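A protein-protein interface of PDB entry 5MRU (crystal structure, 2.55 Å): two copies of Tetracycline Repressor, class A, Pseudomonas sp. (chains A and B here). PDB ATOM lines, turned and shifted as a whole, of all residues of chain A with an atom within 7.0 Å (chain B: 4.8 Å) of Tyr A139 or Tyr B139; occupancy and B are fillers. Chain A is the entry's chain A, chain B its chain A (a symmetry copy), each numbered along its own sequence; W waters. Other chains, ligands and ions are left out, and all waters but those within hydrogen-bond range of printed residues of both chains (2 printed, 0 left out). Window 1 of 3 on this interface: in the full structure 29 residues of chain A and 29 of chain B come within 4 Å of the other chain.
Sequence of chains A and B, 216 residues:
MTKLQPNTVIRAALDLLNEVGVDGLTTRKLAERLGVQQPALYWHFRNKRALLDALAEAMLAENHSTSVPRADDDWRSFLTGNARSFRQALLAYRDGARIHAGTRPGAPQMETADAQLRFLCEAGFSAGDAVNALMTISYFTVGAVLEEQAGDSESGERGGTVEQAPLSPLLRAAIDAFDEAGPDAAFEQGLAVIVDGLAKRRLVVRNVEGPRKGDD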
ATOM      1  N   PHE A  86       0.867   9.360 -11.348  1.00  0.00           N
ATOM      2  CA  PHE A  86       0.904  10.158 -12.562  1.00  0.00           C
ATOM      3  C   PHE A  86       2.236  10.906 -12.598  1.00  0.00           C
ATOM      4  O   PHE A  86       3.049  10.691 -13.488  1.00  0.00           O
ATOM      5  CB  PHE A  86      -0.286  11.122 -12.572  1.00  0.00           C
ATOM      6  CG  PHE A  86      -0.381  12.011 -13.810  1.00  0.00           C
ATOM      7  CD1 PHE A  86      -0.176  11.512 -15.071  1.00  0.00           C
ATOM      8  CD2 PHE A  86      -0.750  13.338 -13.686  1.00  0.00           C
ATOM      9  CE1 PHE A  86      -0.295  12.302 -16.191  1.00  0.00           C
ATOM     10  CE2 PHE A  86      -0.867  14.153 -14.805  1.00  0.00           C
ATOM     11  CZ  PHE A  86      -0.637  13.627 -16.070  1.00  0.00           C
ATOM     12  N   ARG A 104      -5.029  14.112 -24.944  1.00  0.00           N
ATOM     13  CA  ARG A 104      -6.333  13.711 -24.441  1.00  0.00           C
ATOM     14  C   ARG A 104      -6.311  12.206 -24.389  1.00  0.00           C
ATOM     15  O   ARG A 104      -5.919  11.555 -25.363  1.00  0.00           O
ATOM     16  CB  ARG A 104      -7.474  14.235 -25.328  1.00  0.00           C
ATOM     17  CG  ARG A 104      -8.079  15.564 -24.862  1.00  0.00           C
ATOM     18  CD  ARG A 104      -6.994  16.545 -24.400  1.00  0.00           C
ATOM     19  NE  ARG A 104      -7.311  17.955 -24.133  1.00  0.00           N
ATOM     20  CZ  ARG A 104      -8.512  18.506 -23.942  1.00  0.00           C
ATOM     21  NH1 ARG A 104      -9.654  17.814 -23.991  1.00  0.00           N
ATOM     22  NH2 ARG A 104      -8.562  19.816 -23.719  1.00  0.00           N
ATOM     23  N   LEU A 134     -10.341  15.387 -11.108  1.00  0.00           N
ATOM     24  CA  LEU A 134      -9.338  14.705 -11.889  1.00  0.00           C
ATOM     25  C   LEU A 134      -8.592  15.762 -12.657  1.00  0.00           C
ATOM     26  O   LEU A 134      -7.369  15.804 -12.649  1.00  0.00           O
ATOM     27  CB  LEU A 134      -9.971  13.654 -12.798  1.00  0.00           C
ATOM     28  CG  LEU A 134     -10.662  12.496 -12.022  1.00  0.00           C
ATOM     29  CD1 LEU A 134     -11.141  11.383 -12.940  1.00  0.00           C
ATOM     30  CD2 LEU A 134      -9.776  11.889 -10.937  1.00  0.00           C
ATOM     31  N   MET A 135      -9.329  16.660 -13.277  1.00  0.00           N
ATOM     32  CA  MET A 135      -8.677  17.697 -14.042  1.00  0.00           C
ATOM     33  C   MET A 135      -7.735  18.505 -13.145  1.00  0.00           C
ATOM     34  O   MET A 135      -6.565  18.673 -13.441  1.00  0.00           O
ATOM     35  CB  MET A 135      -9.713  18.603 -14.737  1.00  0.00           C
ATOM     36  CG  MET A 135      -9.467  18.720 -16.241  1.00  0.00           C
ATOM     37  SD  MET A 135      -9.727  17.172 -17.169  1.00  0.00           S
ATOM     38  CE  MET A 135     -11.486  17.371 -17.514  1.00  0.00           C
ATOM     39  N   THR A 136      -8.256  18.976 -12.026  1.00  0.00           N
ATOM     40  CA  THR A 136      -7.512  19.885 -11.178  1.00  0.00           C
ATOM     41  C   THR A 136      -6.194  19.275 -10.678  1.00  0.00           C
ATOM     42  O   THR A 136      -5.153  19.921 -10.672  1.00  0.00           O
ATOM     43  CB  THR A 136      -8.402  20.317 -10.014  1.00  0.00           C
ATOM     44  OG1 THR A 136      -9.463  21.157 -10.512  1.00  0.00           O
ATOM     45  CG2 THR A 136      -7.605  21.059  -8.978  1.00  0.00           C
ATOM     46  N   ILE A 137      -6.268  18.023 -10.258  1.00  0.00           N
ATOM     47  CA  ILE A 137      -5.106  17.258  -9.847  1.00  0.00           C
ATOM     48  C   ILE A 137      -4.182  17.155 -11.033  1.00  0.00           C
ATOM     49  O   ILE A 137      -2.978  17.395 -10.923  1.00  0.00           O
ATOM     50  CB  ILE A 137      -5.509  15.850  -9.333  1.00  0.00           C
ATOM     51  CG1 ILE A 137      -6.150  15.963  -7.954  1.00  0.00           C
ATOM     52  CG2 ILE A 137      -4.312  14.899  -9.239  1.00  0.00           C
ATOM     53  CD1 ILE A 137      -6.717  14.674  -7.455  1.00  0.00           C
ATOM     54  N   SER A 138      -4.758  16.818 -12.175  1.00  0.00           N
ATOM     55  CA  SER A 138      -4.031  16.761 -13.427  1.00  0.00           C
ATOM     56  C   SER A 138      -3.293  18.089 -13.789  1.00  0.00           C
ATOM     57  O   SER A 138      -2.078  18.119 -14.073  1.00  0.00           O
ATOM     58  CB  SER A 138      -5.012  16.337 -14.500  1.00  0.00           C
ATOM     59  OG  SER A 138      -4.401  16.352 -15.748  1.00  0.00           O
ATOM     60  N   TYR A 139      -4.015  19.193 -13.732  1.00  0.00           N
ATOM     61  CA  TYR A 139      -3.433  20.502 -14.021  1.00  0.00           C
ATOM     62  C   TYR A 139      -2.349  20.894 -13.046  1.00  0.00           C
ATOM     63  O   TYR A 139      -1.311  21.428 -13.461  1.00  0.00           O
ATOM     64  CB  TYR A 139      -4.521  21.539 -14.083  1.00  0.00           C
ATOM     65  CG  TYR A 139      -5.366  21.361 -15.303  1.00  0.00           C
ATOM     66  CD1 TYR A 139      -4.959  20.525 -16.355  1.00  0.00           C
ATOM     67  CD2 TYR A 139      -6.543  22.050 -15.441  1.00  0.00           C
ATOM     68  CE1 TYR A 139      -5.714  20.384 -17.498  1.00  0.00           C
ATOM     69  CE2 TYR A 139      -7.314  21.920 -16.581  1.00  0.00           C
ATOM     70  CZ  TYR A 139      -6.903  21.080 -17.599  1.00  0.00           C
ATOM     71  OH  TYR A 139      -7.682  20.964 -18.739  1.00  0.00           O
ATOM     72  N   PHE A 140      -2.568  20.583 -11.772  1.00  0.00           N
ATOM     73  CA  PHE A 140      -1.601  20.844 -10.725  1.00  0.00           C
ATOM     74  C   PHE A 140      -0.316  20.064 -10.945  1.00  0.00           C
ATOM     75  O   PHE A 140       0.774  20.591 -10.762  1.00  0.00           O
ATOM     76  CB  PHE A 140      -2.164  20.437  -9.365  1.00  0.00           C
ATOM     77  CG  PHE A 140      -1.168  20.538  -8.254  1.00  0.00           C
ATOM     78  CD1 PHE A 140      -0.623  21.757  -7.918  1.00  0.00           C
ATOM     79  CD2 PHE A 140      -0.759  19.412  -7.562  1.00  0.00           C
ATOM     80  CE1 PHE A 140       0.296  21.862  -6.883  1.00  0.00           C
ATOM     81  CE2 PHE A 140       0.166  19.498  -6.516  1.00  0.00           C
ATOM     82  CZ  PHE A 140       0.697  20.727  -6.179  1.00  0.00           C
ATOM     83  N   THR A 141      -0.465  18.795 -11.295  1.00  0.00           N
ATOM     84  CA  THR A 141       0.666  17.875 -11.400  1.00  0.00           C
ATOM     85  C   THR A 141       1.570  18.271 -12.581  1.00  0.00           C
ATOM     86  O   THR A 141       2.778  18.512 -12.429  1.00  0.00           O
ATOM     87  CB  THR A 141       0.144  16.454 -11.582  1.00  0.00           C
ATOM     88  OG1 THR A 141      -0.836  16.191 -10.581  1.00  0.00           O
ATOM     89  CG2 THR A 141       1.243  15.415 -11.458  1.00  0.00           C
ATOM     90  N   VAL A 142       0.954  18.413 -13.746  1.00  0.00           N
ATOM     91  CA  VAL A 142       1.665  18.810 -14.961  1.00  0.00           C
ATOM     92  C   VAL A 142       2.403  20.128 -14.646  1.00  0.00           C
ATOM     93  O   VAL A 142       3.604  20.286 -14.921  1.00  0.00           O
ATOM     94  CB  VAL A 142       0.656  18.955 -16.127  1.00  0.00           C
ATOM     95  CG1 VAL A 142       1.304  19.505 -17.354  1.00  0.00           C
ATOM     96  CG2 VAL A 142       0.050  17.614 -16.470  1.00  0.00           C
ATOM     97  N   GLY A 143       1.687  21.057 -14.011  1.00  0.00           N
ATOM     98  CA  GLY A 143       2.282  22.324 -13.613  1.00  0.00           C
ATOM     99  C   GLY A 143       3.498  22.056 -12.745  1.00  0.00           C
ATOM    100  O   GLY A 143       4.608  22.499 -13.082  1.00  0.00           O
ATOM    101  N   ALA A 144       3.305  21.288 -11.656  1.00  0.00           N
ATOM    102  CA  ALA A 144       4.399  21.076 -10.696  1.00  0.00           C
ATOM    103  C   ALA A 144       5.616  20.437 -11.393  1.00  0.00           C
ATOM    104  O   ALA A 144       6.745  20.908 -11.238  1.00  0.00           O
ATOM    105  CB  ALA A 144       3.959  20.225  -9.545  1.00  0.00           C
ATOM    106  N   VAL A 145       5.370  19.432 -12.220  1.00  0.00           N
ATOM    107  CA  VAL A 145       6.456  18.719 -12.837  1.00  0.00           C
ATOM    108  C   VAL A 145       7.126  19.621 -13.845  1.00  0.00           C
ATOM    109  O   VAL A 145       8.356  19.701 -13.870  1.00  0.00           O
ATOM    110  CB  VAL A 145       5.981  17.438 -13.511  1.00  0.00           C
ATOM    111  CG1 VAL A 145       7.098  16.813 -14.328  1.00  0.00           C
ATOM    112  CG2 VAL A 145       5.457  16.467 -12.458  1.00  0.00           C
ATOM    113  N   GLU A 147       7.570  22.705 -13.802  1.00  0.00           N
ATOM    114  CA  GLU A 147       8.437  23.670 -13.137  1.00  0.00           C
ATOM    115  C   GLU A 147       9.640  22.953 -12.599  1.00  0.00           C
ATOM    116  O   GLU A 147      10.765  23.425 -12.749  1.00  0.00           O
ATOM    117  CB  GLU A 147       7.708  24.438 -12.060  1.00  0.00           C
ATOM    118  CG  GLU A 147       6.577  25.320 -12.592  1.00  0.00           C
ATOM    119  CD  GLU A 147       6.941  26.785 -12.555  1.00  0.00           C
ATOM    120  OE1 GLU A 147       8.158  27.065 -12.575  1.00  0.00           O
ATOM    121  OE2 GLU A 147       6.030  27.641 -12.494  1.00  0.00           O
ATOM    122  N   GLU A 148       9.444  21.771 -12.052  1.00  0.00           N
ATOM    123  CA  GLU A 148      10.604  21.001 -11.628  1.00  0.00           C
ATOM    124  C   GLU A 148      11.571  20.673 -12.783  1.00  0.00           C
ATOM    125  O   GLU A 148      12.773  20.766 -12.626  1.00  0.00           O
ATOM    126  CB  GLU A 148      10.163  19.707 -10.916  1.00  0.00           C
ATOM    127  CG  GLU A 148      11.357  18.803 -10.593  1.00  0.00           C
ATOM    128  CD  GLU A 148      11.051  17.618  -9.704  1.00  0.00           C
ATOM    129  OE1 GLU A 148       9.857  17.331  -9.412  1.00  0.00           O
ATOM    130  OE2 GLU A 148      12.074  16.995  -9.306  1.00  0.00           O
ATOM    131  N   PRO A 183      11.064  19.674  -4.178  1.00  0.00           N
ATOM    132  CA  PRO A 183       9.934  19.635  -5.096  1.00  0.00           C
ATOM    133  C   PRO A 183       8.946  18.528  -4.735  1.00  0.00           C
ATOM    134  O   PRO A 183       7.760  18.665  -5.020  1.00  0.00           O
ATOM    135  CB  PRO A 183      10.585  19.365  -6.459  1.00  0.00           C
ATOM    136  CG  PRO A 183      11.979  19.878  -6.319  1.00  0.00           C
ATOM    137  CD  PRO A 183      12.354  19.615  -4.886  1.00  0.00           C
ATOM    138  N   ALA A 186       6.753  20.199  -1.741  1.00  0.00           N
ATOM    139  CA  ALA A 186       5.912  21.168  -2.456  1.00  0.00           C
ATOM    140  C   ALA A 186       4.768  20.554  -3.245  1.00  0.00           C
ATOM    141  O   ALA A 186       3.659  21.077  -3.265  1.00  0.00           O
ATOM    142  CB  ALA A 186       6.775  21.969  -3.387  1.00  0.00           C
ATOM    143  N   PHE A 187       5.029  19.444  -3.894  1.00  0.00           N
ATOM    144  CA  PHE A 187       3.984  18.800  -4.628  1.00  0.00           C
ATOM    145  C   PHE A 187       3.048  18.188  -3.656  1.00  0.00           C
ATOM    146  O   PHE A 187       1.856  18.464  -3.675  1.00  0.00           O
ATOM    147  CB  PHE A 187       4.538  17.700  -5.495  1.00  0.00           C
ATOM    148  CG  PHE A 187       3.507  16.745  -5.987  1.00  0.00           C
ATOM    149  CD1 PHE A 187       2.753  17.040  -7.101  1.00  0.00           C
ATOM    150  CD2 PHE A 187       3.318  15.538  -5.354  1.00  0.00           C
ATOM    151  CE1 PHE A 187       1.808  16.154  -7.573  1.00  0.00           C
ATOM    152  CE2 PHE A 187       2.375  14.635  -5.823  1.00  0.00           C
ATOM    153  CZ  PHE A 187       1.615  14.947  -6.940  1.00  0.00           C
ATOM    154  N   GLY A 190       0.785  20.678  -1.987  1.00  0.00           N
ATOM    155  CA  GLY A 190      -0.269  21.264  -2.809  1.00  0.00           C
ATOM    156  C   GLY A 190      -1.378  20.258  -3.026  1.00  0.00           C
ATOM    157  O   GLY A 190      -2.558  20.602  -3.038  1.00  0.00           O
ATOM    158  N   ILE A 194      -5.270  20.286  -2.077  1.00  0.00           N
ATOM    159  CA  ILE A 194      -6.266  19.954  -3.073  1.00  0.00           C
ATOM    160  C   ILE A 194      -7.234  18.902  -2.567  1.00  0.00           C
ATOM    161  O   ILE A 194      -8.421  18.990  -2.816  1.00  0.00           O
ATOM    162  CB  ILE A 194      -5.609  19.524  -4.401  1.00  0.00           C
ATOM    163  CG1 ILE A 194      -5.301  20.785  -5.232  1.00  0.00           C
ATOM    164  CG2 ILE A 194      -6.491  18.533  -5.173  1.00  0.00           C
ATOM    165  CD1 ILE A 194      -4.336  20.559  -6.383  1.00  0.00           C
ATOM    166  N   MET B 135       2.741  28.728  -4.113  1.00  0.00           N
ATOM    167  CA  MET B 135       3.297  27.754  -5.022  1.00  0.00           C
ATOM    168  C   MET B 135       2.178  26.936  -5.673  1.00  0.00           C
ATOM    169  O   MET B 135       2.096  26.825  -6.885  1.00  0.00           O
ATOM    170  CB  MET B 135       4.316  26.846  -4.303  1.00  0.00           C
ATOM    171  CG  MET B 135       5.668  26.812  -5.014  1.00  0.00           C
ATOM    172  SD  MET B 135       6.575  28.394  -4.982  1.00  0.00           S
ATOM    173  CE  MET B 135       7.465  28.150  -3.431  1.00  0.00           C
ATOM    174  N   THR B 136       1.298  26.392  -4.852  1.00  0.00           N
ATOM    175  CA  THR B 136       0.292  25.470  -5.336  1.00  0.00           C
ATOM    176  C   THR B 136      -0.619  26.101  -6.398  1.00  0.00           C
ATOM    177  O   THR B 136      -0.931  25.492  -7.415  1.00  0.00           O
ATOM    178  CB  THR B 136      -0.515  24.949  -4.148  1.00  0.00           C
ATOM    179  OG1 THR B 136       0.321  24.098  -3.339  1.00  0.00           O
ATOM    180  CG2 THR B 136      -1.723  24.186  -4.615  1.00  0.00           C
ATOM    181  N   ILE B 137      -1.039  27.327  -6.136  1.00  0.00           N
ATOM    182  CA  ILE B 137      -1.823  28.112  -7.070  1.00  0.00           C
ATOM    183  C   ILE B 137      -0.993  28.306  -8.314  1.00  0.00           C
ATOM    184  O   ILE B 137      -1.469  28.104  -9.433  1.00  0.00           O
ATOM    185  CB  ILE B 137      -2.233  29.478  -6.458  1.00  0.00           C
ATOM    186  CG1 ILE B 137      -3.334  29.274  -5.423  1.00  0.00           C
ATOM    187  CG2 ILE B 137      -2.734  30.465  -7.517  1.00  0.00           C
ATOM    188  CD1 ILE B 137      -3.674  30.516  -4.665  1.00  0.00           C
ATOM    189  N   SER B 138       0.260  28.678  -8.109  1.00  0.00           N
ATOM    190  CA  SER B 138       1.216  28.823  -9.189  1.00  0.00           C
ATOM    191  C   SER B 138       1.372  27.541 -10.068  1.00  0.00           C
ATOM    192  O   SER B 138       1.260  27.568 -11.310  1.00  0.00           O
ATOM    193  CB  SER B 138       2.527  29.264  -8.574  1.00  0.00           C
ATOM    194  OG  SER B 138       3.518  29.332  -9.546  1.00  0.00           O
ATOM    195  N   TYR B 139       1.585  26.410  -9.419  1.00  0.00           N
ATOM    196  CA  TYR B 139       1.722  25.139 -10.126  1.00  0.00           C
ATOM    197  C   TYR B 139       0.470  24.738 -10.868  1.00  0.00           C
ATOM    198  O   TYR B 139       0.555  24.262 -12.008  1.00  0.00           O
ATOM    199  CB  TYR B 139       2.161  24.068  -9.165  1.00  0.00           C
ATOM    200  CG  TYR B 139       3.579  24.276  -8.737  1.00  0.00           C
ATOM    201  CD1 TYR B 139       4.418  25.176  -9.413  1.00  0.00           C
ATOM    202  CD2 TYR B 139       4.105  23.553  -7.699  1.00  0.00           C
ATOM    203  CE1 TYR B 139       5.735  25.346  -9.048  1.00  0.00           C
ATOM    204  CE2 TYR B 139       5.425  23.711  -7.319  1.00  0.00           C
ATOM    205  CZ  TYR B 139       6.231  24.615  -7.986  1.00  0.00           C
ATOM    206  OH  TYR B 139       7.554  24.759  -7.600  1.00  0.00           O
ATOM    207  N   PHE B 140      -0.680  24.978 -10.244  1.00  0.00           N
ATOM    208  CA  PHE B 140      -1.969  24.700 -10.846  1.00  0.00           C
ATOM    209  C   PHE B 140      -2.193  25.535 -12.095  1.00  0.00           C
ATOM    210  O   PHE B 140      -2.693  25.039 -13.097  1.00  0.00           O
ATOM    211  CB  PHE B 140      -3.096  25.019  -9.866  1.00  0.00           C
ATOM    212  CG  PHE B 140      -4.459  24.899 -10.466  1.00  0.00           C
ATOM    213  CD1 PHE B 140      -4.907  23.686 -10.938  1.00  0.00           C
ATOM    214  CD2 PHE B 140      -5.285  26.004 -10.582  1.00  0.00           C
ATOM    215  CE1 PHE B 140      -6.175  23.562 -11.489  1.00  0.00           C
ATOM    216  CE2 PHE B 140      -6.566  25.899 -11.135  1.00  0.00           C
ATOM    217  CZ  PHE B 140      -7.009  24.675 -11.593  1.00  0.00           C
ATOM    218  N   THR B 141      -1.859  26.814 -12.001  1.00  0.00           N
ATOM    219  CA  THR B 141      -2.149  27.777 -13.061  1.00  0.00           C
ATOM    220  C   THR B 141      -1.301  27.472 -14.308  1.00  0.00           C
ATOM    221  O   THR B 141      -1.818  27.267 -15.418  1.00  0.00           O
ATOM    222  CB  THR B 141      -1.863  29.187 -12.554  1.00  0.00           C
ATOM    223  OG1 THR B 141      -2.513  29.364 -11.297  1.00  0.00           O
ATOM    224  CG2 THR B 141      -2.364  30.256 -13.506  1.00  0.00           C
ATOM    225  N   VAL B 142       0.003  27.366 -14.097  1.00  0.00           N
ATOM    226  CA  VAL B 142       0.945  27.055 -15.172  1.00  0.00           C
ATOM    227  C   VAL B 142       0.461  25.750 -15.837  1.00  0.00           C
ATOM    228  O   VAL B 142       0.348  25.649 -17.070  1.00  0.00           O
ATOM    229  CB  VAL B 142       2.374  26.932 -14.588  1.00  0.00           C
ATOM    230  CG1 VAL B 142       3.352  26.466 -15.615  1.00  0.00           C
ATOM    231  CG2 VAL B 142       2.843  28.266 -14.055  1.00  0.00           C
ATOM    232  N   GLY B 143       0.117  24.766 -15.005  1.00  0.00           N
ATOM    233  CA  GLY B 143      -0.403  23.503 -15.507  1.00  0.00           C
ATOM    234  C   GLY B 143      -1.620  23.771 -16.375  1.00  0.00           C
ATOM    235  O   GLY B 143      -1.634  23.385 -17.555  1.00  0.00           O
ATOM    236  N   ALA B 144      -2.619  24.477 -15.812  1.00  0.00           N
ATOM    237  CA  ALA B 144      -3.881  24.680 -16.538  1.00  0.00           C
ATOM    238  C   ALA B 144      -3.627  25.395 -17.880  1.00  0.00           C
ATOM    239  O   ALA B 144      -4.114  24.958 -18.924  1.00  0.00           O
ATOM    240  CB  ALA B 144      -4.864  25.458 -15.718  1.00  0.00           C
ATOM    241  N   GLU B 147      -1.880  23.320 -20.599  1.00  0.00           N
ATOM    242  CA  GLU B 147      -2.749  22.354 -21.260  1.00  0.00           C
ATOM    243  C   GLU B 147      -3.664  23.087 -22.197  1.00  0.00           C
ATOM    244  O   GLU B 147      -3.860  22.663 -23.334  1.00  0.00           O
ATOM    245  CB  GLU B 147      -3.513  21.509 -20.269  1.00  0.00           C
ATOM    246  CG  GLU B 147      -2.621  20.615 -19.407  1.00  0.00           C
ATOM    247  CD  GLU B 147      -2.718  19.164 -19.813  1.00  0.00           C
ATOM    248  OE1 GLU B 147      -3.073  18.928 -20.986  1.00  0.00           O
ATOM    249  OE2 GLU B 147      -2.458  18.274 -18.971  1.00  0.00           O
ATOM    250  N   ALA B 186     -13.147  25.199 -15.917  1.00  0.00           N
ATOM    251  CA  ALA B 186     -12.169  24.237 -15.391  1.00  0.00           C
ATOM    252  C   ALA B 186     -11.082  24.848 -14.524  1.00  0.00           C
ATOM    253  O   ALA B 186     -10.694  24.287 -13.505  1.00  0.00           O
ATOM    254  CB  ALA B 186     -11.530  23.513 -16.542  1.00  0.00           C
HETATM  255  O   HOH W   1       5.771  29.733 -10.854  1.00  0.00           O
HETATM  256  O   HOH W   2      -3.858  16.096 -18.314  1.00  0.00           O
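Thr A136 touches Phe B140, and with the chains exchanged Phe A140 touches Thr B136.
Tyr A139 touches Gly B143, and with the chains exchanged Gly A143 touches Tyr B139.
Phe B140 touches its own counterpart, Phe A140.
Val A142 touches Glu B147, and with the chains exchanged Glu A147 touches Val B142.
12 positions are printed for both chains.
CD1 of Phe B140 touches O of Thr A136, 3.8 Å away.
Tyr A139 touches Tyr B139.
Phe B140 touches Tyr A139 (CE1 to CB, 3.7 Å).
Gly B143 touches Tyr A139 (CA to O, 3.1 Å).
Ala B144 touches Tyr A139.
Phe B140 touches Phe A140.
O of Tyr B139 touches CA of Gly A143, 3.1 Å away.
Ala A144 touches Tyr B139.
CG of Glu A147 touches CE1 of Tyr B139, 3.6 Å away.
Val B142 touches Glu A147.
Of the printed residues of chain B, Thr A136 touches Phe B140.
Of chain B, only Tyr B139, Phe B140, Gly B143, Ala B144 and Glu B147 come within 4 Å of Tyr A139.
Of the printed residues of chain B, Phe A140 touches Thr B136, Tyr B139 and Phe B140.
Of the printed residues of chain B, Val A142 touches Glu B147 (3.6 Å).
Of the printed residues of chain B, Ala A144 touches Tyr B139 (3.8 Å).
Of chain A, only Tyr A139, Phe A140, Gly A143, Ala A144 and Glu A147 come within 4 Å of Tyr B139.
Printed residues of chain A within 4 Å of Gly B143: Tyr A139 and Gly A143.
The nearest residue of chain B that does not touch Tyr A139 is Ala B186 (4.5 Å).
The nearest printed residue of chain B that does not touch Val A142 is Gly B143 (4.5 Å).
Among the printed residues, 16 pairs touch across the chains.
Among the printed residues, no Asp or Glu carboxylate lies within 4 Å of a Lys or Arg side-chain nitrogen of the other chain.
Water W2 bridges the side-chain hydroxyl (OG) of Ser A138 and the side-chain carboxylate (OE2) of Glu B147.
Water W1 lies within hydrogen-bond range of OG of Ser B138 (2.6 Å) and OE2 of Glu A147 (2.7 Å).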
